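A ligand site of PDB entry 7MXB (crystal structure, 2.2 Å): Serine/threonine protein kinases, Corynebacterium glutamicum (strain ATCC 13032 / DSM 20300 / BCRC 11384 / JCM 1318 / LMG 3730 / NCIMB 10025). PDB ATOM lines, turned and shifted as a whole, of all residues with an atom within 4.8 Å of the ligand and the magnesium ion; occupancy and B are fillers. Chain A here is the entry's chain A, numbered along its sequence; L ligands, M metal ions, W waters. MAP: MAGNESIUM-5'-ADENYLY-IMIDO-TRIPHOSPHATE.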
ATOM      1  N   ILE A  59      -2.397  17.512  11.115  1.00  0.00           N
ATOM      2  CA  ILE A  59      -1.571  17.952  12.231  1.00  0.00           C
ATOM      3  C   ILE A  59      -1.028  16.791  13.055  1.00  0.00           C
ATOM      4  O   ILE A  59      -0.067  16.984  13.817  1.00  0.00           O
ATOM      5  CB  ILE A  59      -2.339  18.919  13.149  1.00  0.00           C
ATOM      6  CG1 ILE A  59      -3.546  18.212  13.791  1.00  0.00           C
ATOM      7  CG2 ILE A  59      -2.754  20.176  12.378  1.00  0.00           C
ATOM      8  CD1 ILE A  59      -4.255  19.019  14.863  1.00  0.00           C
ATOM      9  N   ALA A  60      -1.594  15.596  12.919  1.00  0.00           N
ATOM     10  CA  ALA A  60      -1.160  14.438  13.691  1.00  0.00           C
ATOM     11  C   ALA A  60      -1.817  13.196  13.129  1.00  0.00           C
ATOM     12  O   ALA A  60      -2.789  13.267  12.367  1.00  0.00           O
ATOM     13  CB  ALA A  60      -1.492  14.593  15.182  1.00  0.00           C
ATOM     14  N   GLY A  62      -3.194   9.528  14.898  1.00  0.00           N
ATOM     15  CA  GLY A  62      -3.418   8.888  16.179  1.00  0.00           C
ATOM     16  C   GLY A  62      -4.187   7.588  16.055  1.00  0.00           C
ATOM     17  O   GLY A  62      -4.304   7.042  14.952  1.00  0.00           O
ATOM     18  N   GLY A  63      -4.711   7.090  17.175  1.00  0.00           N
ATOM     19  CA  GLY A  63      -5.467   5.849  17.156  1.00  0.00           C
ATOM     20  C   GLY A  63      -6.672   5.920  16.238  1.00  0.00           C
ATOM     21  O   GLY A  63      -7.005   4.945  15.557  1.00  0.00           O
ATOM     22  N   MET A  64      -7.348   7.057  16.210  1.00  0.00           N
ATOM     23  CA  MET A  64      -8.515   7.244  15.345  1.00  0.00           C
ATOM     24  C   MET A  64      -8.135   7.571  13.899  1.00  0.00           C
ATOM     25  O   MET A  64      -9.037   7.775  13.079  1.00  0.00           O
ATOM     26  CB  MET A  64      -9.426   8.326  15.920  1.00  0.00           C
ATOM     27  CG  MET A  64      -9.999   7.993  17.298  1.00  0.00           C
ATOM     28  SD  MET A  64     -10.987   6.481  17.318  1.00  0.00           S
ATOM     29  CE  MET A  64     -12.235   6.847  16.089  1.00  0.00           C
ATOM     30  N   GLY A  65      -6.848   7.639  13.578  1.00  0.00           N
ATOM     31  CA  GLY A  65      -6.410   7.944  12.225  1.00  0.00           C
ATOM     32  C   GLY A  65      -5.815   9.341  12.117  1.00  0.00           C
ATOM     33  O   GLY A  65      -5.409   9.962  13.112  1.00  0.00           O
ATOM     34  N   ILE A  67      -5.530  13.279  11.739  1.00  0.00           N
ATOM     35  CA  ILE A  67      -6.267  14.405  12.321  1.00  0.00           C
ATOM     36  C   ILE A  67      -6.041  15.612  11.416  1.00  0.00           C
ATOM     37  O   ILE A  67      -4.910  16.118  11.310  1.00  0.00           O
ATOM     38  CB  ILE A  67      -5.821  14.692  13.761  1.00  0.00           C
ATOM     39  CG1 ILE A  67      -5.911  13.425  14.610  1.00  0.00           C
ATOM     40  CG2 ILE A  67      -6.663  15.797  14.356  1.00  0.00           C
ATOM     41  CD1 ILE A  67      -5.433  13.613  16.046  1.00  0.00           C
ATOM     42  N   VAL A  81     -10.634  21.313  13.835  1.00  0.00           N
ATOM     43  CA  VAL A  81     -10.016  19.989  13.773  1.00  0.00           C
ATOM     44  C   VAL A  81     -11.065  18.985  13.327  1.00  0.00           C
ATOM     45  O   VAL A  81     -12.213  19.013  13.793  1.00  0.00           O
ATOM     46  CB  VAL A  81      -9.439  19.612  15.154  1.00  0.00           C
ATOM     47  CG1 VAL A  81      -9.193  18.118  15.247  1.00  0.00           C
ATOM     48  CG2 VAL A  81      -8.151  20.371  15.423  1.00  0.00           C
ATOM     49  N   LYS A  83     -11.505  15.042  13.449  1.00  0.00           N
ATOM     50  CA  LYS A  83     -10.955  13.861  14.114  1.00  0.00           C
ATOM     51  C   LYS A  83     -11.934  12.704  13.977  1.00  0.00           C
ATOM     52  O   LYS A  83     -13.146  12.897  14.074  1.00  0.00           O
ATOM     53  CB  LYS A  83     -10.681  14.139  15.585  1.00  0.00           C
ATOM     54  CG  LYS A  83     -10.083  12.978  16.354  1.00  0.00           C
ATOM     55  CD  LYS A  83      -9.791  13.373  17.790  1.00  0.00           C
ATOM     56  CE  LYS A  83      -9.240  12.215  18.594  1.00  0.00           C
ATOM     57  NZ  LYS A  83      -8.845  12.655  19.960  1.00  0.00           N
ATOM     58  N   VAL A 113     -12.482  21.502  25.152  1.00  0.00           N
ATOM     59  CA  VAL A 113     -12.570  21.882  23.743  1.00  0.00           C
ATOM     60  C   VAL A 113     -14.030  21.825  23.299  1.00  0.00           C
ATOM     61  O   VAL A 113     -14.801  20.963  23.727  1.00  0.00           O
ATOM     62  CB  VAL A 113     -11.669  20.976  22.891  1.00  0.00           C
ATOM     63  CG1 VAL A 113     -12.241  19.563  22.798  1.00  0.00           C
ATOM     64  CG2 VAL A 113     -11.488  21.562  21.509  1.00  0.00           C
ATOM     65  N   MET A 131     -14.121  19.851  15.912  1.00  0.00           N
ATOM     66  CA  MET A 131     -13.921  20.510  17.188  1.00  0.00           C
ATOM     67  C   MET A 131     -12.961  21.687  17.053  1.00  0.00           C
ATOM     68  O   MET A 131     -12.263  21.841  16.047  1.00  0.00           O
ATOM     69  CB  MET A 131     -13.407  19.525  18.251  1.00  0.00           C
ATOM     70  CG  MET A 131     -12.108  18.838  17.880  1.00  0.00           C
ATOM     71  SD  MET A 131     -11.532  17.755  19.193  1.00  0.00           S
ATOM     72  CE  MET A 131     -12.625  16.362  19.001  1.00  0.00           C
ATOM     73  N   GLU A 132     -12.950  22.522  18.087  1.00  0.00           N
ATOM     74  CA  GLU A 132     -12.054  23.658  18.163  1.00  0.00           C
ATOM     75  C   GLU A 132     -10.598  23.216  18.104  1.00  0.00           C
ATOM     76  O   GLU A 132     -10.213  22.195  18.674  1.00  0.00           O
ATOM     77  CB  GLU A 132     -12.332  24.427  19.461  1.00  0.00           C
ATOM     78  CG  GLU A 132     -11.166  25.223  20.025  1.00  0.00           C
ATOM     79  CD  GLU A 132     -11.396  25.617  21.470  1.00  0.00           C
ATOM     80  OE1 GLU A 132     -12.454  25.261  22.026  1.00  0.00           O
ATOM     81  OE2 GLU A 132     -10.511  26.271  22.055  1.00  0.00           O
ATOM     82  N   TYR A 133      -9.779  23.985  17.372  1.00  0.00           N
ATOM     83  CA  TYR A 133      -8.342  23.752  17.331  1.00  0.00           C
ATOM     84  C   TYR A 133      -7.681  24.468  18.502  1.00  0.00           C
ATOM     85  O   TYR A 133      -7.798  25.688  18.636  1.00  0.00           O
ATOM     86  CB  TYR A 133      -7.747  24.214  16.012  1.00  0.00           C
ATOM     87  CG  TYR A 133      -6.230  24.153  16.014  1.00  0.00           C
ATOM     88  CD1 TYR A 133      -5.569  22.930  15.971  1.00  0.00           C
ATOM     89  CD2 TYR A 133      -5.464  25.306  16.094  1.00  0.00           C
ATOM     90  CE1 TYR A 133      -4.197  22.857  15.982  1.00  0.00           C
ATOM     91  CE2 TYR A 133      -4.089  25.240  16.116  1.00  0.00           C
ATOM     92  CZ  TYR A 133      -3.451  24.016  16.055  1.00  0.00           C
ATOM     93  OH  TYR A 133      -2.076  23.950  16.077  1.00  0.00           O
ATOM     94  N   VAL A 134      -6.987  23.709  19.345  1.00  0.00           N
ATOM     95  CA  VAL A 134      -6.301  24.242  20.514  1.00  0.00           C
ATOM     96  C   VAL A 134      -4.816  24.334  20.173  1.00  0.00           C
ATOM     97  O   VAL A 134      -4.158  23.316  19.952  1.00  0.00           O
ATOM     98  CB  VAL A 134      -6.535  23.363  21.751  1.00  0.00           C
ATOM     99  CG1 VAL A 134      -6.025  24.056  22.991  1.00  0.00           C
ATOM    100  CG2 VAL A 134      -8.009  23.031  21.883  1.00  0.00           C
ATOM    101  N   SER A 138       0.817  19.277  24.013  1.00  0.00           N
ATOM    102  CA  SER A 138       0.195  18.448  25.024  1.00  0.00           C
ATOM    103  C   SER A 138       1.139  18.283  26.209  1.00  0.00           C
ATOM    104  O   SER A 138       2.352  18.520  26.108  1.00  0.00           O
ATOM    105  CB  SER A 138      -0.159  17.076  24.461  1.00  0.00           C
ATOM    106  OG  SER A 138       0.987  16.253  24.400  1.00  0.00           O
ATOM    107  N   ASP A 179     -10.963   9.172  29.245  1.00  0.00           N
ATOM    108  CA  ASP A 179      -9.673   8.932  28.596  1.00  0.00           C
ATOM    109  C   ASP A 179      -8.615   9.966  28.987  1.00  0.00           C
ATOM    110  O   ASP A 179      -7.759  10.333  28.192  1.00  0.00           O
ATOM    111  CB  ASP A 179      -9.823   8.899  27.078  1.00  0.00           C
ATOM    112  CG  ASP A 179      -8.655   8.214  26.389  1.00  0.00           C
ATOM    113  OD1 ASP A 179      -7.980   7.376  27.030  1.00  0.00           O
ATOM    114  OD2 ASP A 179      -8.389   8.531  25.206  1.00  0.00           O
ATOM    115  N   LYS A 181      -5.315  11.465  29.948  1.00  0.00           N
ATOM    116  CA  LYS A 181      -3.915  11.088  29.835  1.00  0.00           C
ATOM    117  C   LYS A 181      -3.152  12.300  29.291  1.00  0.00           C
ATOM    118  O   LYS A 181      -3.764  13.201  28.732  1.00  0.00           O
ATOM    119  CB  LYS A 181      -3.720   9.858  28.922  1.00  0.00           C
ATOM    120  CG  LYS A 181      -4.348   9.973  27.546  1.00  0.00           C
ATOM    121  CD  LYS A 181      -4.160   8.690  26.745  1.00  0.00           C
ATOM    122  CE  LYS A 181      -4.812   8.777  25.376  1.00  0.00           C
ATOM    123  NZ  LYS A 181      -4.518   7.596  24.528  1.00  0.00           N
ATOM    124  N   GLU A 183      -1.524  13.103  26.725  1.00  0.00           N
ATOM    125  CA  GLU A 183      -1.548  13.488  25.323  1.00  0.00           C
ATOM    126  C   GLU A 183      -2.841  14.174  24.901  1.00  0.00           C
ATOM    127  O   GLU A 183      -2.889  14.731  23.798  1.00  0.00           O
ATOM    128  CB  GLU A 183      -1.287  12.269  24.438  1.00  0.00           C
ATOM    129  CG  GLU A 183      -2.445  11.282  24.324  1.00  0.00           C
ATOM    130  CD  GLU A 183      -2.076  10.046  23.509  1.00  0.00           C
ATOM    131  OE1 GLU A 183      -0.923   9.571  23.620  1.00  0.00           O
ATOM    132  OE2 GLU A 183      -2.929   9.556  22.754  1.00  0.00           O
ATOM    133  N   ASN A 184      -3.894  14.158  25.720  1.00  0.00           N
ATOM    134  CA  ASN A 184      -5.094  14.935  25.415  1.00  0.00           C
ATOM    135  C   ASN A 184      -5.326  16.070  26.422  1.00  0.00           C
ATOM    136  O   ASN A 184      -6.444  16.567  26.560  1.00  0.00           O
ATOM    137  CB  ASN A 184      -6.328  14.039  25.295  1.00  0.00           C
ATOM    138  CG  ASN A 184      -6.542  13.133  26.494  1.00  0.00           C
ATOM    139  OD1 ASN A 184      -6.551  13.583  27.636  1.00  0.00           O
ATOM    140  ND2 ASN A 184      -6.720  11.847  26.235  1.00  0.00           N
ATOM    141  N   ILE A 186      -3.821  19.818  26.760  1.00  0.00           N
ATOM    142  CA  ILE A 186      -3.021  20.797  26.047  1.00  0.00           C
ATOM    143  C   ILE A 186      -2.860  22.044  26.905  1.00  0.00           C
ATOM    144  O   ILE A 186      -3.841  22.574  27.442  1.00  0.00           O
ATOM    145  CB  ILE A 186      -3.633  21.146  24.682  1.00  0.00           C
ATOM    146  CG1 ILE A 186      -3.411  20.000  23.693  1.00  0.00           C
ATOM    147  CG2 ILE A 186      -3.021  22.424  24.134  1.00  0.00           C
ATOM    148  CD1 ILE A 186      -3.795  20.343  22.269  1.00  0.00           C
ATOM    149  N   ILE A 195      -9.097  17.929  25.441  1.00  0.00           N
ATOM    150  CA  ILE A 195      -9.409  17.900  24.019  1.00  0.00           C
ATOM    151  C   ILE A 195     -10.110  16.622  23.576  1.00  0.00           C
ATOM    152  O   ILE A 195     -10.662  16.592  22.460  1.00  0.00           O
ATOM    153  CB  ILE A 195      -8.167  18.137  23.144  1.00  0.00           C
ATOM    154  CG1 ILE A 195      -7.167  16.995  23.309  1.00  0.00           C
ATOM    155  CG2 ILE A 195      -7.527  19.485  23.474  1.00  0.00           C
ATOM    156  CD1 ILE A 195      -5.983  17.079  22.373  1.00  0.00           C
ATOM    157  N   ASP A 196     -10.107  15.554  24.371  1.00  0.00           N
ATOM    158  CA  ASP A 196     -10.673  14.273  23.947  1.00  0.00           C
ATOM    159  C   ASP A 196     -12.172  14.220  24.268  1.00  0.00           C
ATOM    160  O   ASP A 196     -12.642  13.412  25.066  1.00  0.00           O
ATOM    161  CB  ASP A 196      -9.926  13.116  24.592  1.00  0.00           C
ATOM    162  CG  ASP A 196     -10.115  11.807  23.856  1.00  0.00           C
ATOM    163  OD1 ASP A 196     -10.907  11.767  22.890  1.00  0.00           O
ATOM    164  OD2 ASP A 196      -9.480  10.812  24.248  1.00  0.00           O
ATOM    165  N   TYR A 210     -13.985   3.780  25.543  1.00  0.00           N
ATOM    166  CA  TYR A 210     -12.735   4.050  24.850  1.00  0.00           C
ATOM    167  C   TYR A 210     -11.687   4.704  25.761  1.00  0.00           C
ATOM    168  O   TYR A 210     -11.212   5.818  25.536  1.00  0.00           O
ATOM    169  CB  TYR A 210     -12.998   4.901  23.614  1.00  0.00           C
ATOM    170  CG  TYR A 210     -13.569   4.110  22.459  1.00  0.00           C
ATOM    171  CD1 TYR A 210     -12.735   3.486  21.532  1.00  0.00           C
ATOM    172  CD2 TYR A 210     -14.948   3.978  22.289  1.00  0.00           C
ATOM    173  CE1 TYR A 210     -13.251   2.755  20.480  1.00  0.00           C
ATOM    174  CE2 TYR A 210     -15.474   3.249  21.238  1.00  0.00           C
ATOM    175  CZ  TYR A 210     -14.624   2.635  20.343  1.00  0.00           C
ATOM    176  OH  TYR A 210     -15.138   1.914  19.292  1.00  0.00           O
ATOM    177  N   THR A 212      -7.834   4.069  27.838  1.00  0.00           N
ATOM    178  CA  THR A 212      -6.493   3.688  27.410  1.00  0.00           C
ATOM    179  C   THR A 212      -5.900   2.716  28.428  1.00  0.00           C
ATOM    180  O   THR A 212      -5.804   3.050  29.618  1.00  0.00           O
ATOM    181  CB  THR A 212      -5.580   4.902  27.246  1.00  0.00           C
ATOM    182  OG1 THR A 212      -6.149   5.805  26.282  1.00  0.00           O
ATOM    183  CG2 THR A 212      -4.191   4.478  26.774  1.00  0.00           C
HETATM  184  PG  MAP L   1      -6.594   7.872  21.368  1.00  0.00           P
HETATM  185  O1G MAP L   1      -5.394   8.380  22.069  1.00  0.00           O
HETATM  186  O2G MAP L   1      -6.178   6.550  20.560  1.00  0.00           O
HETATM  187  O3G MAP L   1      -7.731   7.517  22.445  1.00  0.00           O
HETATM  188  PB  MAP L   1      -6.215   9.601  19.120  1.00  0.00           P
HETATM  189  O1B MAP L   1      -4.872   8.963  19.117  1.00  0.00           O
HETATM  190  O2B MAP L   1      -6.931   9.338  17.696  1.00  0.00           O
HETATM  191  N3B MAP L   1      -7.144   9.015  20.334  1.00  0.00           N
HETATM  192  PA  MAP L   1      -5.631  12.072  20.575  1.00  0.00           P
HETATM  193  O1A MAP L   1      -6.776  12.538  21.387  1.00  0.00           O
HETATM  194  O2A MAP L   1      -4.735  11.198  21.407  1.00  0.00           O
HETATM  195  O3A MAP L   1      -6.128  11.189  19.332  1.00  0.00           O
HETATM  196  O5' MAP L   1      -4.739  13.286  19.991  1.00  0.00           O
HETATM  197  C5' MAP L   1      -3.513  13.040  19.335  1.00  0.00           C
HETATM  198  C4' MAP L   1      -2.794  14.372  19.162  1.00  0.00           C
HETATM  199  O4' MAP L   1      -3.486  15.165  18.203  1.00  0.00           O
HETATM  200  C3' MAP L   1      -2.830  15.189  20.431  1.00  0.00           C
HETATM  201  O3' MAP L   1      -1.726  14.890  21.296  1.00  0.00           O
HETATM  202  C2' MAP L   1      -2.797  16.644  19.989  1.00  0.00           C
HETATM  203  O2' MAP L   1      -1.435  17.026  19.786  1.00  0.00           O
HETATM  204  C1' MAP L   1      -3.467  16.535  18.628  1.00  0.00           C
HETATM  205  N9  MAP L   1      -4.868  17.018  18.734  1.00  0.00           N
HETATM  206  C8  MAP L   1      -5.956  16.248  18.858  1.00  0.00           C
HETATM  207  N7  MAP L   1      -7.057  17.027  18.936  1.00  0.00           N
HETATM  208  C5  MAP L   1      -6.643  18.309  18.868  1.00  0.00           C
HETATM  209  C6  MAP L   1      -7.350  19.617  18.902  1.00  0.00           C
HETATM  210  N6  MAP L   1      -8.699  19.679  19.021  1.00  0.00           N
HETATM  211  N1  MAP L   1      -6.618  20.750  18.816  1.00  0.00           N
HETATM  212  C2  MAP L   1      -5.294  20.622  18.694  1.00  0.00           C
HETATM  213  N3  MAP L   1      -4.595  19.483  18.658  1.00  0.00           N
HETATM  214  C4  MAP L   1      -5.254  18.302  18.748  1.00  0.00           C
HETATM  215 MG   MAP L   1      -3.919   9.532  20.726  1.00  0.00          MG
HETATM  216 MG    MG M   1      -8.697   9.152  23.376  1.00  0.00          MG
HETATM  217  O   HOH W   1       1.095  15.042  21.904  1.00  0.00           O
HETATM  218  O   HOH W   2      -6.865  10.257  15.010  1.00  0.00           O
HETATM  219  O   HOH W   3      -2.048  10.102  20.197  1.00  0.00           O
HETATM  220  O   HOH W   4      -2.864   7.639  21.025  1.00  0.00           O
HETATM  221  O   HOH W   5       0.808  15.420  18.186  1.00  0.00           O
HETATM  222  O   HOH W   6      -9.614   9.941  21.581  1.00  0.00           O
HETATM  223  O   HOH W   7      -1.255  11.304  17.890  1.00  0.00           O
HETATM  224  O   HOH W   8     -10.455   8.102  23.489  1.00  0.00           O
HETATM  225  O   HOH W   9      -9.504  15.403  20.206  1.00  0.00           O
HETATM  226  O   HOH W  10      -8.783   4.527  20.321  1.00  0.00           O
HETATM  227  O   HOH W  11      -7.058  10.441  23.245  1.00  0.00           O
HETATM  228  O   HOH W  12      -2.095  19.854  18.219  1.00  0.00           O
HETATM  229  O   HOH W  13       0.075  19.742  19.959  1.00  0.00           O
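The backbone carbonyl oxygen of Glu 183 lies within hydrogen-bond range of an oxygen (O3') of the ligand.
A magnesium atom (MG) of the ligand is bound by the side-chain carboxylate (OE2) of Glu 183, at 2.3 Å.
The side-chain amino group (NZ) of Lys 83 is in salt-bridge range of an oxygen (O1A) of the ligand (2.5 Å).
An oxygen (O2B) of the ligand lies within hydrogen-bond range of the backbone NH of Gly 63 (3.2 Å).
An oxygen (O3G) of the ligand sits close to the side-chain amino group (NZ) of Lys 181.
N of Met 64 lies within hydrogen-bond range of O2B of the ligand.
N6 of the ligand lies within hydrogen-bond range of O of Glu 132.
A nitrogen (N1) of the ligand is in hydrogen-bond range of the backbone NH of Val 134 (3.0 Å).
A nitrogen (N6) of the ligand lies within hydrogen-bond range of the side-chain sulfur (SD) of Met 131, 3.4 Å away.
CD1 of Ile 59 touches N3 of the ligand, at 3.8 Å.
CB of Ala 60 touches O4' of the ligand, 3.7 Å away.
Gly 62 touches the ligand (CA to O1B, 3.3 Å).
CD1 of Ile 67 touches O4' of the ligand, 3.3 Å away.
Val 81 touches the ligand.
CD1 of Tyr 133 touches C2 of the ligand (3.6 Å).
CD1 of Ile 186 touches N3 of the ligand, 3.8 Å away.
CD1 of Ile 195 touches N7 of the ligand, 3.6 Å away.
Hydrophobic or aromatic side chains that line the ligand: Ile 59, Ala 60, Met 64, Ile 67, Val 81, Met 131, Tyr 133, Val 134, Ile 186 and Ile 195.
Of the 24 residues printed, 17 come within 4 Å of the ligand.
The nearest printed residue that does not touch the ligand is Asp 196 (4.1 Å).
The magnesium ion is bound by OD2 of Asp 179 (2.0 Å), OD2 of Asp 196 (2.0 Å), water W8 (2.1 Å), water W11 (2.1 Å), O3G of the ligand (2.1 Å) and water W6 (2.2 Å).
The magnesium ion has six donor atoms within binding distance.
Two residues have an atom within 4 Å of the magnesium ion: Asp 179 and Asp 196.
The nearest printed residue that does not touch the magnesium ion is Lys 181 (4.4 Å).
ND2 of Asn 184 sits at hydrogen-bond distance from O of Asp 179 (2.7 Å).
The side-chain carboxylate (OD1) of Asp 179 is in hydrogen-bond range of the side-chain hydroxyl (OG1) of Thr 212 (2.5 Å).
OE2 of Glu 183 sits close to NZ of Lys 181, 3.1 Å away.
The side-chain amide oxygen (OD1) of Asn 184 sits close to the backbone carbonyl oxygen (O) of Lys 181 (3.0 Å).
The side-chain hydroxyl (OG1) of Thr 212 sits at hydrogen-bond distance from the side-chain amino group (NZ) of Lys 181.
N of Ile 67 sits at hydrogen-bond distance from O of Ala 60.
The backbone NH (N) of Ile 59 lies within hydrogen-bond range of the backbone carbonyl oxygen (O) of Ile 67 (2.9 Å).
O of Met 131 lies within hydrogen-bond range of N of Val 81.
Water W6 lies within hydrogen-bond range of OD1 of Asp 196, N3B of the ligand and NZ of Lys 83.
Water W11 bridges an oxygen (O1A) of the ligand and the side-chain amide nitrogen of Asn 184.
Water W2 lies within hydrogen-bond range of O of Gly 65 (2.4 Å), O2B of the ligand (2.8 Å) and N of Met 64 (3.5 Å).
Water W1 lies within hydrogen-bond range of the side-chain hydroxyl of Ser 138 (2.8 Å) and an oxygen (O3') of the ligand (2.9 Å).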
